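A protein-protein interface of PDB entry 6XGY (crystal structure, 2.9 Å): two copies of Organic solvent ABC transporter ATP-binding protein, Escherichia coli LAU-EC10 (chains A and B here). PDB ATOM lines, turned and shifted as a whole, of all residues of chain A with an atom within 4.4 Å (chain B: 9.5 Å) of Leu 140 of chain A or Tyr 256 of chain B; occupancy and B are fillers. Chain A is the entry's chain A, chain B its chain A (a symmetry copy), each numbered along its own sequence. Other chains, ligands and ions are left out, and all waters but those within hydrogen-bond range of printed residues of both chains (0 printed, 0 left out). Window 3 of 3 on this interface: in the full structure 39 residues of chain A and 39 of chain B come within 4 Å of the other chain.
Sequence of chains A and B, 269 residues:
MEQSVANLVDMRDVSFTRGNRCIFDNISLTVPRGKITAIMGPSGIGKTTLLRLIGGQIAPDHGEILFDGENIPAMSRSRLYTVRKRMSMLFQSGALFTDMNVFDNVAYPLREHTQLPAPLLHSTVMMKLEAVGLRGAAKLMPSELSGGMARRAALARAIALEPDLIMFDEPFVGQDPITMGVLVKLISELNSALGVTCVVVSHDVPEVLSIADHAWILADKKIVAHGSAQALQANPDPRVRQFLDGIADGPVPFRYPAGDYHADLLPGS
N of Tyr 256 of chain B lies within hydrogen-bond range of O of Gly 133 of chain A (3.1 Å).
Tyr 256 of chain B touches five residues of chain A. No residue of chain B comes within 4 Å of Asn 101 of chain A. Gly 136 of chain A touches just these residues of chain B: Tyr 256, Pro 257 and Ala 258. Of the printed residues of chain B, Ala 137 of chain A touches Tyr 256 (3.6 Å). Of the printed residues of chain B, Gly 133 of chain A touches Phe 254 (3.5 Å), Arg 255 (3.5 Å) and Tyr 256 (3.1 Å). Of the printed residues of chain A, Ala 258 of chain B touches Gly 136. Printed residues of chain B within 4 Å of Met 149 of chain A: Tyr 256 (3.8 Å). Printed residues of chain A within 4 Å of Phe 254 of chain B: Gly 133 (3.5 Å). Leu 145 of chain A touches none of the printed residues of chain B. Val 102 of chain A touches none of the printed residues of chain B. The nearest printed residue of chain B that does not touch Gly 133 of chain A is Pro 257 of chain B (6.3 Å).
Printed residues of chain B that touch a printed residue of chain A: Phe 254, Arg 255, Tyr 256, Pro 257 and Ala 258. Hydrophobic or aromatic side chains of chain B that line the printed part of chain A: Phe 254, Tyr 256 and Ala 258. Of the 12 printed residues of chain A, 5 touch a printed residue of chain B.
No position is printed for both chains. Of the 9 pairs that touch across the chains among the printed residues, none has its exchanged pair printed and touching as well.
Among the printed residues, merely in contact across the chains: Gly 136 of chain A with Tyr 256 of chain B, Gly 136 of chain A with Pro 257 of chain B, Gly 133 of chain A with Arg 255 of chain B, Gly 136 of chain A with Ala 258 of chain B, Gly 133 of chain A with Phe 254 of chain B, Ala 137 of chain A with Tyr 256 of chain B, Met 149 of chain A with Tyr 256 of chain B and Leu 140 of chain A with Tyr 256 of chain B.
The backbone carbonyl oxygen (O) of Leu 140 of chain A lies within hydrogen-bond range of the backbone NH (N) of Val 102 of chain A (3.0 Å). The side-chain carboxylate (OD2) of Asp 249 of chain B lies within hydrogen-bond range of the backbone NH (N) of Phe 254 of chain B.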
ATOM      1  N   ASN A 101     -14.294  -1.680   6.199  1.00  0.00           N
ATOM      2  CA  ASN A 101     -12.869  -1.919   6.395  1.00  0.00           C
ATOM      3  C   ASN A 101     -12.314  -0.994   7.484  1.00  0.00           C
ATOM      4  O   ASN A 101     -13.043  -0.247   8.143  1.00  0.00           O
ATOM      5  CB  ASN A 101     -12.127  -1.767   5.068  1.00  0.00           C
ATOM      6  CG  ASN A 101     -12.362  -0.420   4.409  1.00  0.00           C
ATOM      7  OD1 ASN A 101     -12.246   0.628   5.044  1.00  0.00           O
ATOM      8  ND2 ASN A 101     -12.696  -0.442   3.124  1.00  0.00           N
ATOM      9  N   VAL A 102     -10.993  -1.043   7.673  1.00  0.00           N
ATOM     10  CA  VAL A 102     -10.357  -0.313   8.769  1.00  0.00           C
ATOM     11  C   VAL A 102     -10.372   1.186   8.504  1.00  0.00           C
ATOM     12  O   VAL A 102     -10.649   1.988   9.406  1.00  0.00           O
ATOM     13  CB  VAL A 102      -8.924  -0.830   8.989  1.00  0.00           C
ATOM     14  CG1 VAL A 102      -8.213  -0.004  10.058  1.00  0.00           C
ATOM     15  CG2 VAL A 102      -8.943  -2.306   9.365  1.00  0.00           C
ATOM     16  N   GLY A 133       0.175   2.707  13.636  1.00  0.00           N
ATOM     17  CA  GLY A 133       0.939   1.801  12.799  1.00  0.00           C
ATOM     18  C   GLY A 133       0.121   0.802  12.014  1.00  0.00           C
ATOM     19  O   GLY A 133       0.561  -0.337  11.828  1.00  0.00           O
ATOM     20  N   GLY A 136      -0.972   0.238   6.638  1.00  0.00           N
ATOM     21  CA  GLY A 136      -0.997  -0.843   5.670  1.00  0.00           C
ATOM     22  C   GLY A 136      -2.229  -1.717   5.756  1.00  0.00           C
ATOM     23  O   GLY A 136      -2.559  -2.403   4.783  1.00  0.00           O
ATOM     24  N   ALA A 137      -2.917  -1.710   6.897  1.00  0.00           N
ATOM     25  CA  ALA A 137      -4.129  -2.490   7.091  1.00  0.00           C
ATOM     26  C   ALA A 137      -5.392  -1.694   6.790  1.00  0.00           C
ATOM     27  O   ALA A 137      -6.474  -2.070   7.253  1.00  0.00           O
ATOM     28  CB  ALA A 137      -4.182  -3.035   8.519  1.00  0.00           C
ATOM     29  N   ALA A 138      -5.278  -0.609   6.019  1.00  0.00           N
ATOM     30  CA  ALA A 138      -6.418   0.281   5.821  1.00  0.00           C
ATOM     31  C   ALA A 138      -7.544  -0.399   5.052  1.00  0.00           C
ATOM     32  O   ALA A 138      -8.717  -0.055   5.238  1.00  0.00           O
ATOM     33  CB  ALA A 138      -5.973   1.553   5.098  1.00  0.00           C
ATOM     34  N   LYS A 139      -7.216  -1.353   4.185  1.00  0.00           N
ATOM     35  CA  LYS A 139      -8.222  -2.057   3.402  1.00  0.00           C
ATOM     36  C   LYS A 139      -8.630  -3.385   4.018  1.00  0.00           C
ATOM     37  O   LYS A 139      -9.551  -4.031   3.507  1.00  0.00           O
ATOM     38  CB  LYS A 139      -7.724  -2.272   1.972  1.00  0.00           C
ATOM     39  CG  LYS A 139      -8.109  -1.143   1.034  1.00  0.00           C
ATOM     40  CD  LYS A 139      -7.537  -1.342  -0.356  1.00  0.00           C
ATOM     41  CE  LYS A 139      -8.025  -0.258  -1.305  1.00  0.00           C
ATOM     42  NZ  LYS A 139      -7.473  -0.440  -2.676  1.00  0.00           N
ATOM     43  N   LEU A 140      -7.979  -3.805   5.099  1.00  0.00           N
ATOM     44  CA  LEU A 140      -8.363  -5.027   5.786  1.00  0.00           C
ATOM     45  C   LEU A 140      -9.694  -4.836   6.514  1.00  0.00           C
ATOM     46  O   LEU A 140     -10.203  -3.723   6.662  1.00  0.00           O
ATOM     47  CB  LEU A 140      -7.280  -5.454   6.775  1.00  0.00           C
ATOM     48  CG  LEU A 140      -6.173  -6.388   6.283  1.00  0.00           C
ATOM     49  CD1 LEU A 140      -5.329  -5.730   5.202  1.00  0.00           C
ATOM     50  CD2 LEU A 140      -5.305  -6.835   7.453  1.00  0.00           C
ATOM     51  N   MET A 141     -10.254  -5.947   6.971  1.00  0.00           N
ATOM     52  CA  MET A 141     -11.485  -5.979   7.741  1.00  0.00           C
ATOM     53  C   MET A 141     -11.200  -6.399   9.177  1.00  0.00           C
ATOM     54  O   MET A 141     -10.166  -7.014   9.460  1.00  0.00           O
ATOM     55  CB  MET A 141     -12.489  -6.958   7.114  1.00  0.00           C
ATOM     56  CG  MET A 141     -12.742  -6.743   5.629  1.00  0.00           C
ATOM     57  SD  MET A 141     -13.810  -5.336   5.278  1.00  0.00           S
ATOM     58  CE  MET A 141     -15.305  -5.819   6.135  1.00  0.00           C
ATOM     59  N   GLU A 144     -10.204 -10.086   9.658  1.00  0.00           N
ATOM     60  CA  GLU A 144      -8.826 -10.512   9.471  1.00  0.00           C
ATOM     61  C   GLU A 144      -7.879  -9.968  10.528  1.00  0.00           C
ATOM     62  O   GLU A 144      -6.747 -10.456  10.631  1.00  0.00           O
ATOM     63  CB  GLU A 144      -8.333 -10.076   8.087  1.00  0.00           C
ATOM     64  CG  GLU A 144      -9.372 -10.204   6.990  1.00  0.00           C
ATOM     65  CD  GLU A 144      -8.877  -9.674   5.659  1.00  0.00           C
ATOM     66  OE1 GLU A 144      -9.447  -8.679   5.159  1.00  0.00           O
ATOM     67  OE2 GLU A 144      -7.909 -10.247   5.118  1.00  0.00           O
ATOM     68  N   LEU A 145      -8.305  -8.978  11.308  1.00  0.00           N
ATOM     69  CA  LEU A 145      -7.394  -8.299  12.219  1.00  0.00           C
ATOM     70  C   LEU A 145      -6.924  -9.223  13.331  1.00  0.00           C
ATOM     71  O   LEU A 145      -7.680 -10.062  13.828  1.00  0.00           O
ATOM     72  CB  LEU A 145      -8.062  -7.070  12.829  1.00  0.00           C
ATOM     73  CG  LEU A 145      -8.094  -5.835  11.935  1.00  0.00           C
ATOM     74  CD1 LEU A 145      -8.522  -4.613  12.730  1.00  0.00           C
ATOM     75  CD2 LEU A 145      -6.737  -5.611  11.282  1.00  0.00           C
ATOM     76  N   MET A 149      -3.929  -5.956  16.920  1.00  0.00           N
ATOM     77  CA  MET A 149      -4.173  -5.055  15.796  1.00  0.00           C
ATOM     78  C   MET A 149      -5.597  -4.518  15.803  1.00  0.00           C
ATOM     79  O   MET A 149      -5.831  -3.371  15.405  1.00  0.00           O
ATOM     80  CB  MET A 149      -3.883  -5.764  14.471  1.00  0.00           C
ATOM     81  CG  MET A 149      -2.405  -5.859  14.127  1.00  0.00           C
ATOM     82  SD  MET A 149      -2.079  -6.925  12.709  1.00  0.00           S
ATOM     83  CE  MET A 149      -2.961  -6.065  11.409  1.00  0.00           C
ATOM     84  N   ASP B 249       8.824  -2.060  19.032  1.00  0.00           N
ATOM     85  CA  ASP B 249       9.281  -2.336  17.679  1.00  0.00           C
ATOM     86  C   ASP B 249      10.529  -3.208  17.707  1.00  0.00           C
ATOM     87  O   ASP B 249      11.420  -3.015  18.540  1.00  0.00           O
ATOM     88  CB  ASP B 249       9.553  -1.036  16.912  1.00  0.00           C
ATOM     89  CG  ASP B 249       9.599  -1.246  15.411  1.00  0.00           C
ATOM     90  OD1 ASP B 249      10.708  -1.234  14.838  1.00  0.00           O
ATOM     91  OD2 ASP B 249       8.522  -1.441  14.805  1.00  0.00           O
ATOM     92  N   VAL B 252       9.380  -8.158  15.349  1.00  0.00           N
ATOM     93  CA  VAL B 252       7.932  -8.069  15.190  1.00  0.00           C
ATOM     94  C   VAL B 252       7.599  -6.598  14.975  1.00  0.00           C
ATOM     95  O   VAL B 252       7.566  -5.824  15.943  1.00  0.00           O
ATOM     96  CB  VAL B 252       7.191  -8.648  16.405  1.00  0.00           C
ATOM     97  CG1 VAL B 252       5.691  -8.457  16.247  1.00  0.00           C
ATOM     98  CG2 VAL B 252       7.529 -10.119  16.576  1.00  0.00           C
ATOM     99  N   PRO B 253       7.364  -6.168  13.737  1.00  0.00           N
ATOM    100  CA  PRO B 253       7.223  -4.731  13.471  1.00  0.00           C
ATOM    101  C   PRO B 253       5.997  -4.140  14.146  1.00  0.00           C
ATOM    102  O   PRO B 253       4.926  -4.749  14.187  1.00  0.00           O
ATOM    103  CB  PRO B 253       7.102  -4.663  11.943  1.00  0.00           C
ATOM    104  CG  PRO B 253       7.671  -5.952  11.450  1.00  0.00           C
ATOM    105  CD  PRO B 253       7.330  -6.964  12.501  1.00  0.00           C
ATOM    106  N   PHE B 254       6.170  -2.934  14.687  1.00  0.00           N
ATOM    107  CA  PHE B 254       5.021  -2.164  15.143  1.00  0.00           C
ATOM    108  C   PHE B 254       4.178  -1.687  13.969  1.00  0.00           C
ATOM    109  O   PHE B 254       2.953  -1.572  14.092  1.00  0.00           O
ATOM    110  CB  PHE B 254       5.489  -0.980  15.994  1.00  0.00           C
ATOM    111  CG  PHE B 254       4.534   0.182  16.004  1.00  0.00           C
ATOM    112  CD1 PHE B 254       3.319   0.098  16.663  1.00  0.00           C
ATOM    113  CD2 PHE B 254       4.860   1.367  15.362  1.00  0.00           C
ATOM    114  CE1 PHE B 254       2.443   1.168  16.670  1.00  0.00           C
ATOM    115  CE2 PHE B 254       3.990   2.439  15.367  1.00  0.00           C
ATOM    116  CZ  PHE B 254       2.780   2.341  16.023  1.00  0.00           C
ATOM    117  N   ARG B 255       4.803  -1.434  12.823  1.00  0.00           N
ATOM    118  CA  ARG B 255       4.119  -0.873  11.667  1.00  0.00           C
ATOM    119  C   ARG B 255       3.822  -1.961  10.643  1.00  0.00           C
ATOM    120  O   ARG B 255       4.719  -2.708  10.240  1.00  0.00           O
ATOM    121  CB  ARG B 255       4.950   0.240  11.028  1.00  0.00           C
ATOM    122  CG  ARG B 255       5.199   1.414  11.958  1.00  0.00           C
ATOM    123  CD  ARG B 255       5.384   2.717  11.201  1.00  0.00           C
ATOM    124  NE  ARG B 255       5.544   3.845  12.115  1.00  0.00           N
ATOM    125  CZ  ARG B 255       4.539   4.582  12.577  1.00  0.00           C
ATOM    126  NH1 ARG B 255       3.294   4.311  12.207  1.00  0.00           N
ATOM    127  NH2 ARG B 255       4.777   5.589  13.407  1.00  0.00           N
ATOM    128  N   TYR B 256       2.561  -2.045  10.238  1.00  0.00           N
ATOM    129  CA  TYR B 256       2.174  -2.928   9.151  1.00  0.00           C
ATOM    130  C   TYR B 256       2.773  -2.417   7.841  1.00  0.00           C
ATOM    131  O   TYR B 256       2.781  -1.207   7.597  1.00  0.00           O
ATOM    132  CB  TYR B 256       0.647  -2.985   9.054  1.00  0.00           C
ATOM    133  CG  TYR B 256       0.077  -4.201   8.357  1.00  0.00           C
ATOM    134  CD1 TYR B 256      -0.119  -5.392   9.045  1.00  0.00           C
ATOM    135  CD2 TYR B 256      -0.295  -4.148   7.021  1.00  0.00           C
ATOM    136  CE1 TYR B 256      -0.652  -6.503   8.416  1.00  0.00           C
ATOM    137  CE2 TYR B 256      -0.829  -5.253   6.382  1.00  0.00           C
ATOM    138  CZ  TYR B 256      -1.004  -6.428   7.085  1.00  0.00           C
ATOM    139  OH  TYR B 256      -1.535  -7.531   6.454  1.00  0.00           O
ATOM    140  N   PRO B 257       3.301  -3.301   6.993  1.00  0.00           N
ATOM    141  CA  PRO B 257       3.857  -2.843   5.710  1.00  0.00           C
ATOM    142  C   PRO B 257       2.793  -2.134   4.882  1.00  0.00           C
ATOM    143  O   PRO B 257       1.710  -2.672   4.640  1.00  0.00           O
ATOM    144  CB  PRO B 257       4.332  -4.142   5.045  1.00  0.00           C
ATOM    145  CG  PRO B 257       4.528  -5.101   6.181  1.00  0.00           C
ATOM    146  CD  PRO B 257       3.461  -4.752   7.180  1.00  0.00           C
ATOM    147  N   ALA B 258       3.109  -0.912   4.452  1.00  0.00           N
ATOM    148  CA  ALA B 258       2.095  -0.023   3.901  1.00  0.00           C
ATOM    149  C   ALA B 258       2.425   0.492   2.508  1.00  0.00           C
ATOM    150  O   ALA B 258       1.517   0.753   1.717  1.00  0.00           O
ATOM    151  CB  ALA B 258       1.881   1.172   4.835  1.00  0.00           C
ATOM    152  N   GLY B 259       3.707   0.659   2.197  1.00  0.00           N
ATOM    153  CA  GLY B 259       4.070   1.277   0.940  1.00  0.00           C
ATOM    154  C   GLY B 259       4.370   2.753   1.094  1.00  0.00           C
ATOM    155  O   GLY B 259       4.765   3.202   2.174  1.00  0.00           O
ATOM    156  N   ASP B 260       4.172   3.523   0.027  1.00  0.00           N
ATOM    157  CA  ASP B 260       4.595   4.917   0.011  1.00  0.00           C
ATOM    158  C   ASP B 260       3.613   5.778   0.798  1.00  0.00           C
ATOM    159  O   ASP B 260       2.428   5.856   0.457  1.00  0.00           O
ATOM    160  CB  ASP B 260       4.718   5.423  -1.422  1.00  0.00           C
ATOM    161  CG  ASP B 260       5.375   6.782  -1.494  1.00  0.00           C
ATOM    162  OD1 ASP B 260       6.546   6.896  -1.075  1.00  0.00           O
ATOM    163  OD2 ASP B 260       4.724   7.739  -1.959  1.00  0.00           O
ATOM    164  N   ASP B 264      -0.261   8.165  -0.125  1.00  0.00           N
ATOM    165  CA  ASP B 264      -1.490   7.960   0.638  1.00  0.00           C
ATOM    166  C   ASP B 264      -2.031   9.265   1.203  1.00  0.00           C
ATOM    167  O   ASP B 264      -3.243   9.391   1.414  1.00  0.00           O
ATOM    168  CB  ASP B 264      -1.257   6.960   1.769  1.00  0.00           C
ATOM    169  CG  ASP B 264      -1.216   5.526   1.280  1.00  0.00           C
ATOM    170  OD1 ASP B 264      -1.767   5.251   0.191  1.00  0.00           O
ATOM    171  OD2 ASP B 264      -0.640   4.672   1.988  1.00  0.00           O
